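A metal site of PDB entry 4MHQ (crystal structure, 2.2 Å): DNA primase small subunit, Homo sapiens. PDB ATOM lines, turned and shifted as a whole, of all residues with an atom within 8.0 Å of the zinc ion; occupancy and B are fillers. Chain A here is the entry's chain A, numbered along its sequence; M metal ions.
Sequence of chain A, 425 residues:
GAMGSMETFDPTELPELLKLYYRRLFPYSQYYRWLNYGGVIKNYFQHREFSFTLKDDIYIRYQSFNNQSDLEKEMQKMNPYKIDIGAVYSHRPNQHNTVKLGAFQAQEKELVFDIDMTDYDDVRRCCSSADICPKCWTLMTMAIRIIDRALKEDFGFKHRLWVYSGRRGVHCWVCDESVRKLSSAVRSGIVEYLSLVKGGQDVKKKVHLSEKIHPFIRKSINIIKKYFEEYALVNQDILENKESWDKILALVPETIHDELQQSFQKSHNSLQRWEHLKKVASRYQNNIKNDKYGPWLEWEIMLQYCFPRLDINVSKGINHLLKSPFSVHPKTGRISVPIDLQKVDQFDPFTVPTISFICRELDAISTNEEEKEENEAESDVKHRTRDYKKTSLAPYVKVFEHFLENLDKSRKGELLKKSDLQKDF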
ATOM      1  N   MET A 117      17.258   3.821  24.464  1.00  0.00           N
ATOM      2  CA  MET A 117      17.759   5.109  24.948  1.00  0.00           C
ATOM      3  C   MET A 117      19.219   5.081  25.462  1.00  0.00           C
ATOM      4  O   MET A 117      19.935   6.079  25.328  1.00  0.00           O
ATOM      5  CB  MET A 117      16.819   5.712  26.000  1.00  0.00           C
ATOM      6  CG  MET A 117      17.124   7.156  26.384  1.00  0.00           C
ATOM      7  SD  MET A 117      16.862   8.347  25.041  1.00  0.00           S
ATOM      8  CE  MET A 117      15.145   8.787  25.331  1.00  0.00           C
ATOM      9  N   ARG A 124      23.821  12.170  25.560  1.00  0.00           N
ATOM     10  CA  ARG A 124      22.813  12.657  26.509  1.00  0.00           C
ATOM     11  C   ARG A 124      23.480  13.250  27.731  1.00  0.00           C
ATOM     12  O   ARG A 124      24.495  12.721  28.223  1.00  0.00           O
ATOM     13  CB  ARG A 124      21.929  11.516  27.029  1.00  0.00           C
ATOM     14  CG  ARG A 124      20.920  10.940  26.074  1.00  0.00           C
ATOM     15  CD  ARG A 124      20.531   9.577  26.620  1.00  0.00           C
ATOM     16  NE  ARG A 124      19.512   9.713  27.652  1.00  0.00           N
ATOM     17  CZ  ARG A 124      19.295   8.865  28.645  1.00  0.00           C
ATOM     18  NH1 ARG A 124      20.042   7.774  28.807  1.00  0.00           N
ATOM     19  NH2 ARG A 124      18.320   9.121  29.491  1.00  0.00           N
ATOM     20  N   ARG A 125      22.877  14.308  28.255  1.00  0.00           N
ATOM     21  CA  ARG A 125      23.418  15.077  29.374  1.00  0.00           C
ATOM     22  C   ARG A 125      22.379  15.316  30.451  1.00  0.00           C
ATOM     23  O   ARG A 125      22.699  15.839  31.503  1.00  0.00           O
ATOM     24  CB  ARG A 125      23.903  16.427  28.875  1.00  0.00           C
ATOM     25  CG  ARG A 125      25.312  16.436  28.331  1.00  0.00           C
ATOM     26  CD  ARG A 125      25.602  17.739  27.600  1.00  0.00           C
ATOM     27  NE  ARG A 125      24.940  18.886  28.219  1.00  0.00           N
ATOM     28  CZ  ARG A 125      25.444  19.617  29.214  1.00  0.00           C
ATOM     29  NH1 ARG A 125      26.619  19.315  29.745  1.00  0.00           N
ATOM     30  NH2 ARG A 125      24.756  20.653  29.683  1.00  0.00           N
ATOM     31  N   CYS A 126      21.140  14.930  30.170  1.00  0.00           N
ATOM     32  CA  CYS A 126      19.984  15.359  30.955  1.00  0.00           C
ATOM     33  C   CYS A 126      19.746  14.609  32.266  1.00  0.00           C
ATOM     34  O   CYS A 126      19.924  15.180  33.346  1.00  0.00           O
ATOM     35  CB  CYS A 126      18.723  15.344  30.087  1.00  0.00           C
ATOM     36  SG  CYS A 126      18.557  13.827  29.118  1.00  0.00           S
ATOM     37  N   CYS A 127      19.341  13.345  32.208  1.00  0.00           N
ATOM     38  CA  CYS A 127      18.902  12.670  33.425  1.00  0.00           C
ATOM     39  C   CYS A 127      19.902  11.674  33.988  1.00  0.00           C
ATOM     40  O   CYS A 127      20.605  11.973  34.957  1.00  0.00           O
ATOM     41  CB  CYS A 127      17.487  12.071  33.282  1.00  0.00           C
ATOM     42  SG  CYS A 127      17.221  11.111  31.782  1.00  0.00           S
ATOM     43  N   SER A 128      19.950  10.483  33.403  1.00  0.00           N
ATOM     44  CA  SER A 128      20.875   9.430  33.830  1.00  0.00           C
ATOM     45  C   SER A 128      20.722   8.233  32.920  1.00  0.00           C
ATOM     46  O   SER A 128      19.720   8.116  32.222  1.00  0.00           O
ATOM     47  CB  SER A 128      20.621   9.028  35.292  1.00  0.00           C
ATOM     48  OG  SER A 128      19.446   8.236  35.424  1.00  0.00           O
ATOM     49  N   SER A 129      21.705   7.340  32.963  1.00  0.00           N
ATOM     50  CA  SER A 129      21.725   6.160  32.106  1.00  0.00           C
ATOM     51  C   SER A 129      20.505   5.259  32.269  1.00  0.00           C
ATOM     52  O   SER A 129      20.026   4.686  31.287  1.00  0.00           O
ATOM     53  CB  SER A 129      23.017   5.374  32.318  1.00  0.00           C
ATOM     54  OG  SER A 129      23.186   4.391  31.303  1.00  0.00           O
ATOM     55  N   ASP A 131      17.488   6.206  33.230  1.00  0.00           N
ATOM     56  CA  ASP A 131      16.275   7.025  33.153  1.00  0.00           C
ATOM     57  C   ASP A 131      15.970   7.534  31.736  1.00  0.00           C
ATOM     58  O   ASP A 131      16.815   7.480  30.842  1.00  0.00           O
ATOM     59  CB  ASP A 131      16.429   8.256  34.050  1.00  0.00           C
ATOM     60  CG  ASP A 131      15.974   8.018  35.463  1.00  0.00           C
ATOM     61  OD1 ASP A 131      14.764   7.774  35.669  1.00  0.00           O
ATOM     62  OD2 ASP A 131      16.827   8.098  36.370  1.00  0.00           O
ATOM     63  N   ILE A 132      14.744   8.034  31.578  1.00  0.00           N
ATOM     64  CA  ILE A 132      14.391   8.927  30.476  1.00  0.00           C
ATOM     65  C   ILE A 132      13.724  10.170  31.081  1.00  0.00           C
ATOM     66  O   ILE A 132      13.299  10.140  32.239  1.00  0.00           O
ATOM     67  CB  ILE A 132      13.494   8.253  29.408  1.00  0.00           C
ATOM     68  CG1 ILE A 132      12.181   7.738  30.028  1.00  0.00           C
ATOM     69  CG2 ILE A 132      14.233   7.114  28.726  1.00  0.00           C
ATOM     70  CD1 ILE A 132      11.106   7.411  28.999  1.00  0.00           C
ATOM     71  N   CYS A 133      13.643  11.252  30.328  1.00  0.00           N
ATOM     72  CA  CYS A 133      13.005  12.481  30.792  1.00  0.00           C
ATOM     73  C   CYS A 133      12.488  13.254  29.580  1.00  0.00           C
ATOM     74  O   CYS A 133      12.882  12.944  28.453  1.00  0.00           O
ATOM     75  CB  CYS A 133      13.992  13.329  31.610  1.00  0.00           C
ATOM     76  SG  CYS A 133      15.216  14.180  30.608  1.00  0.00           S
ATOM     77  N   PRO A 134      11.599  14.252  29.791  1.00  0.00           N
ATOM     78  CA  PRO A 134      11.086  15.059  28.664  1.00  0.00           C
ATOM     79  C   PRO A 134      12.191  15.687  27.805  1.00  0.00           C
ATOM     80  O   PRO A 134      11.920  16.074  26.668  1.00  0.00           O
ATOM     81  CB  PRO A 134      10.286  16.165  29.366  1.00  0.00           C
ATOM     82  CG  PRO A 134       9.844  15.532  30.644  1.00  0.00           C
ATOM     83  CD  PRO A 134      10.977  14.654  31.073  1.00  0.00           C
ATOM     84  N   LYS A 135      13.414  15.773  28.323  1.00  0.00           N
ATOM     85  CA  LYS A 135      14.551  16.380  27.609  1.00  0.00           C
ATOM     86  C   LYS A 135      15.239  15.423  26.654  1.00  0.00           C
ATOM     87  O   LYS A 135      15.775  15.845  25.637  1.00  0.00           O
ATOM     88  CB  LYS A 135      15.586  16.956  28.581  1.00  0.00           C
ATOM     89  CG  LYS A 135      15.086  18.158  29.367  1.00  0.00           C
ATOM     90  CD  LYS A 135      16.178  18.719  30.259  1.00  0.00           C
ATOM     91  CE  LYS A 135      15.631  19.852  31.104  1.00  0.00           C
ATOM     92  NZ  LYS A 135      16.686  20.857  31.390  1.00  0.00           N
ATOM     93  N   CYS A 136      15.255  14.132  26.969  1.00  0.00           N
ATOM     94  CA  CYS A 136      15.816  13.184  26.026  1.00  0.00           C
ATOM     95  C   CYS A 136      14.772  12.468  25.180  1.00  0.00           C
ATOM     96  O   CYS A 136      15.122  11.927  24.128  1.00  0.00           O
ATOM     97  CB  CYS A 136      16.792  12.192  26.680  1.00  0.00           C
ATOM     98  SG  CYS A 136      16.128  11.325  28.115  1.00  0.00           S
ATOM     99  N   TRP A 137      13.503  12.478  25.595  1.00  0.00           N
ATOM    100  CA  TRP A 137      12.471  11.752  24.842  1.00  0.00           C
ATOM    101  C   TRP A 137      12.441  12.124  23.350  1.00  0.00           C
ATOM    102  O   TRP A 137      12.183  11.274  22.508  1.00  0.00           O
ATOM    103  CB  TRP A 137      11.059  11.855  25.453  1.00  0.00           C
ATOM    104  CG  TRP A 137      10.117  10.928  24.728  1.00  0.00           C
ATOM    105  CD1 TRP A 137       9.134  11.285  23.838  1.00  0.00           C
ATOM    106  CD2 TRP A 137      10.150   9.492  24.741  1.00  0.00           C
ATOM    107  NE1 TRP A 137       8.525  10.152  23.339  1.00  0.00           N
ATOM    108  CE2 TRP A 137       9.128   9.043  23.867  1.00  0.00           C
ATOM    109  CE3 TRP A 137      10.922   8.532  25.426  1.00  0.00           C
ATOM    110  CZ2 TRP A 137       8.870   7.680  23.648  1.00  0.00           C
ATOM    111  CZ3 TRP A 137      10.658   7.180  25.212  1.00  0.00           C
ATOM    112  CH2 TRP A 137       9.631   6.755  24.339  1.00  0.00           C
ATOM    113  N   LEU A 139      14.609  12.401  21.319  1.00  0.00           N
ATOM    114  CA  LEU A 139      15.456  11.455  20.579  1.00  0.00           C
ATOM    115  C   LEU A 139      14.627  10.336  19.972  1.00  0.00           C
ATOM    116  O   LEU A 139      14.857   9.926  18.824  1.00  0.00           O
ATOM    117  CB  LEU A 139      16.541  10.846  21.486  1.00  0.00           C
ATOM    118  CG  LEU A 139      17.710  11.760  21.851  1.00  0.00           C
ATOM    119  CD1 LEU A 139      18.561  11.149  22.969  1.00  0.00           C
ATOM    120  CD2 LEU A 139      18.568  12.056  20.614  1.00  0.00           C
ATOM    121  N   TYR A 231      15.839  20.939  21.093  1.00  0.00           N
ATOM    122  CA  TYR A 231      16.343  19.713  21.708  1.00  0.00           C
ATOM    123  C   TYR A 231      17.790  19.826  22.178  1.00  0.00           C
ATOM    124  O   TYR A 231      18.119  19.495  23.318  1.00  0.00           O
ATOM    125  CB  TYR A 231      16.195  18.474  20.815  1.00  0.00           C
ATOM    126  CG  TYR A 231      17.034  17.339  21.328  1.00  0.00           C
ATOM    127  CD1 TYR A 231      16.663  16.614  22.460  1.00  0.00           C
ATOM    128  CD2 TYR A 231      18.261  17.010  20.717  1.00  0.00           C
ATOM    129  CE1 TYR A 231      17.455  15.599  22.962  1.00  0.00           C
ATOM    130  CE2 TYR A 231      19.059  16.005  21.228  1.00  0.00           C
ATOM    131  CZ  TYR A 231      18.651  15.298  22.345  1.00  0.00           C
ATOM    132  OH  TYR A 231      19.444  14.300  22.852  1.00  0.00           O
ATOM    133  N   GLN A 236      19.167  20.016  25.977  1.00  0.00           N
ATOM    134  CA  GLN A 236      20.404  19.318  26.330  1.00  0.00           C
ATOM    135  C   GLN A 236      21.502  20.316  26.671  1.00  0.00           C
ATOM    136  O   GLN A 236      22.371  20.016  27.493  1.00  0.00           O
ATOM    137  CB  GLN A 236      20.871  18.390  25.196  1.00  0.00           C
ATOM    138  CG  GLN A 236      19.997  17.163  24.977  1.00  0.00           C
ATOM    139  CD  GLN A 236      20.010  16.183  26.145  1.00  0.00           C
ATOM    140  OE1 GLN A 236      21.065  15.827  26.659  1.00  0.00           O
ATOM    141  NE2 GLN A 236      18.827  15.735  26.562  1.00  0.00           N
ATOM    142  N   PHE A 350       5.309   9.102  29.830  1.00  0.00           N
ATOM    143  CA  PHE A 350       5.182   9.256  31.290  1.00  0.00           C
ATOM    144  C   PHE A 350       3.756   9.128  31.808  1.00  0.00           C
ATOM    145  O   PHE A 350       3.552   8.831  32.971  1.00  0.00           O
ATOM    146  CB  PHE A 350       5.808  10.555  31.754  1.00  0.00           C
ATOM    147  CG  PHE A 350       7.217  10.745  31.274  1.00  0.00           C
ATOM    148  CD1 PHE A 350       8.256   9.990  31.811  1.00  0.00           C
ATOM    149  CD2 PHE A 350       7.495  11.644  30.244  1.00  0.00           C
ATOM    150  CE1 PHE A 350       9.566  10.148  31.355  1.00  0.00           C
ATOM    151  CE2 PHE A 350       8.800  11.809  29.783  1.00  0.00           C
ATOM    152  CZ  PHE A 350       9.830  11.068  30.335  1.00  0.00           C
HETATM  153 ZN    ZN M   1      16.802  12.576  30.000  1.00  0.00          ZN
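The side-chain amide nitrogen (NE2) of Gln 236 lies close to the side-chain sulfur (SG) of Cys 126 (3.2 Å).
N of Lys 135 sits close to SG of Cys 133 (3.3 Å).
SG of Cys 127 sits close to NH2 of Arg 124 (3.2 Å).
The side-chain sulfur (SG) of Cys 127 lies close to the backbone carbonyl oxygen (O) of Asp 131.
The side-chain sulfur of Cys 136 sits close to the guanidinium group of Arg 124 (3.4 Å).
O of Ser 128 sits at hydrogen-bond distance from NH2 of Arg 124 (3.2 Å).
O of Asp 131 lies within hydrogen-bond range of NH2 of Arg 124, at 2.6 Å.
Merely in contact with the zinc ion: Arg 124 (3.8 Å).
Of the 18 residues printed, 5 come within 4 Å of the zinc ion.
The zinc ion is bound by the side-chain sulfur of Cys 126 (2.3 Å), the side-chain sulfur of Cys 133 (2.3 Å), the side-chain sulfur of Cys 127 (2.3 Å) and the side-chain sulfur of Cys 136 (2.4 Å).
The zinc ion has four donor atoms within binding distance.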
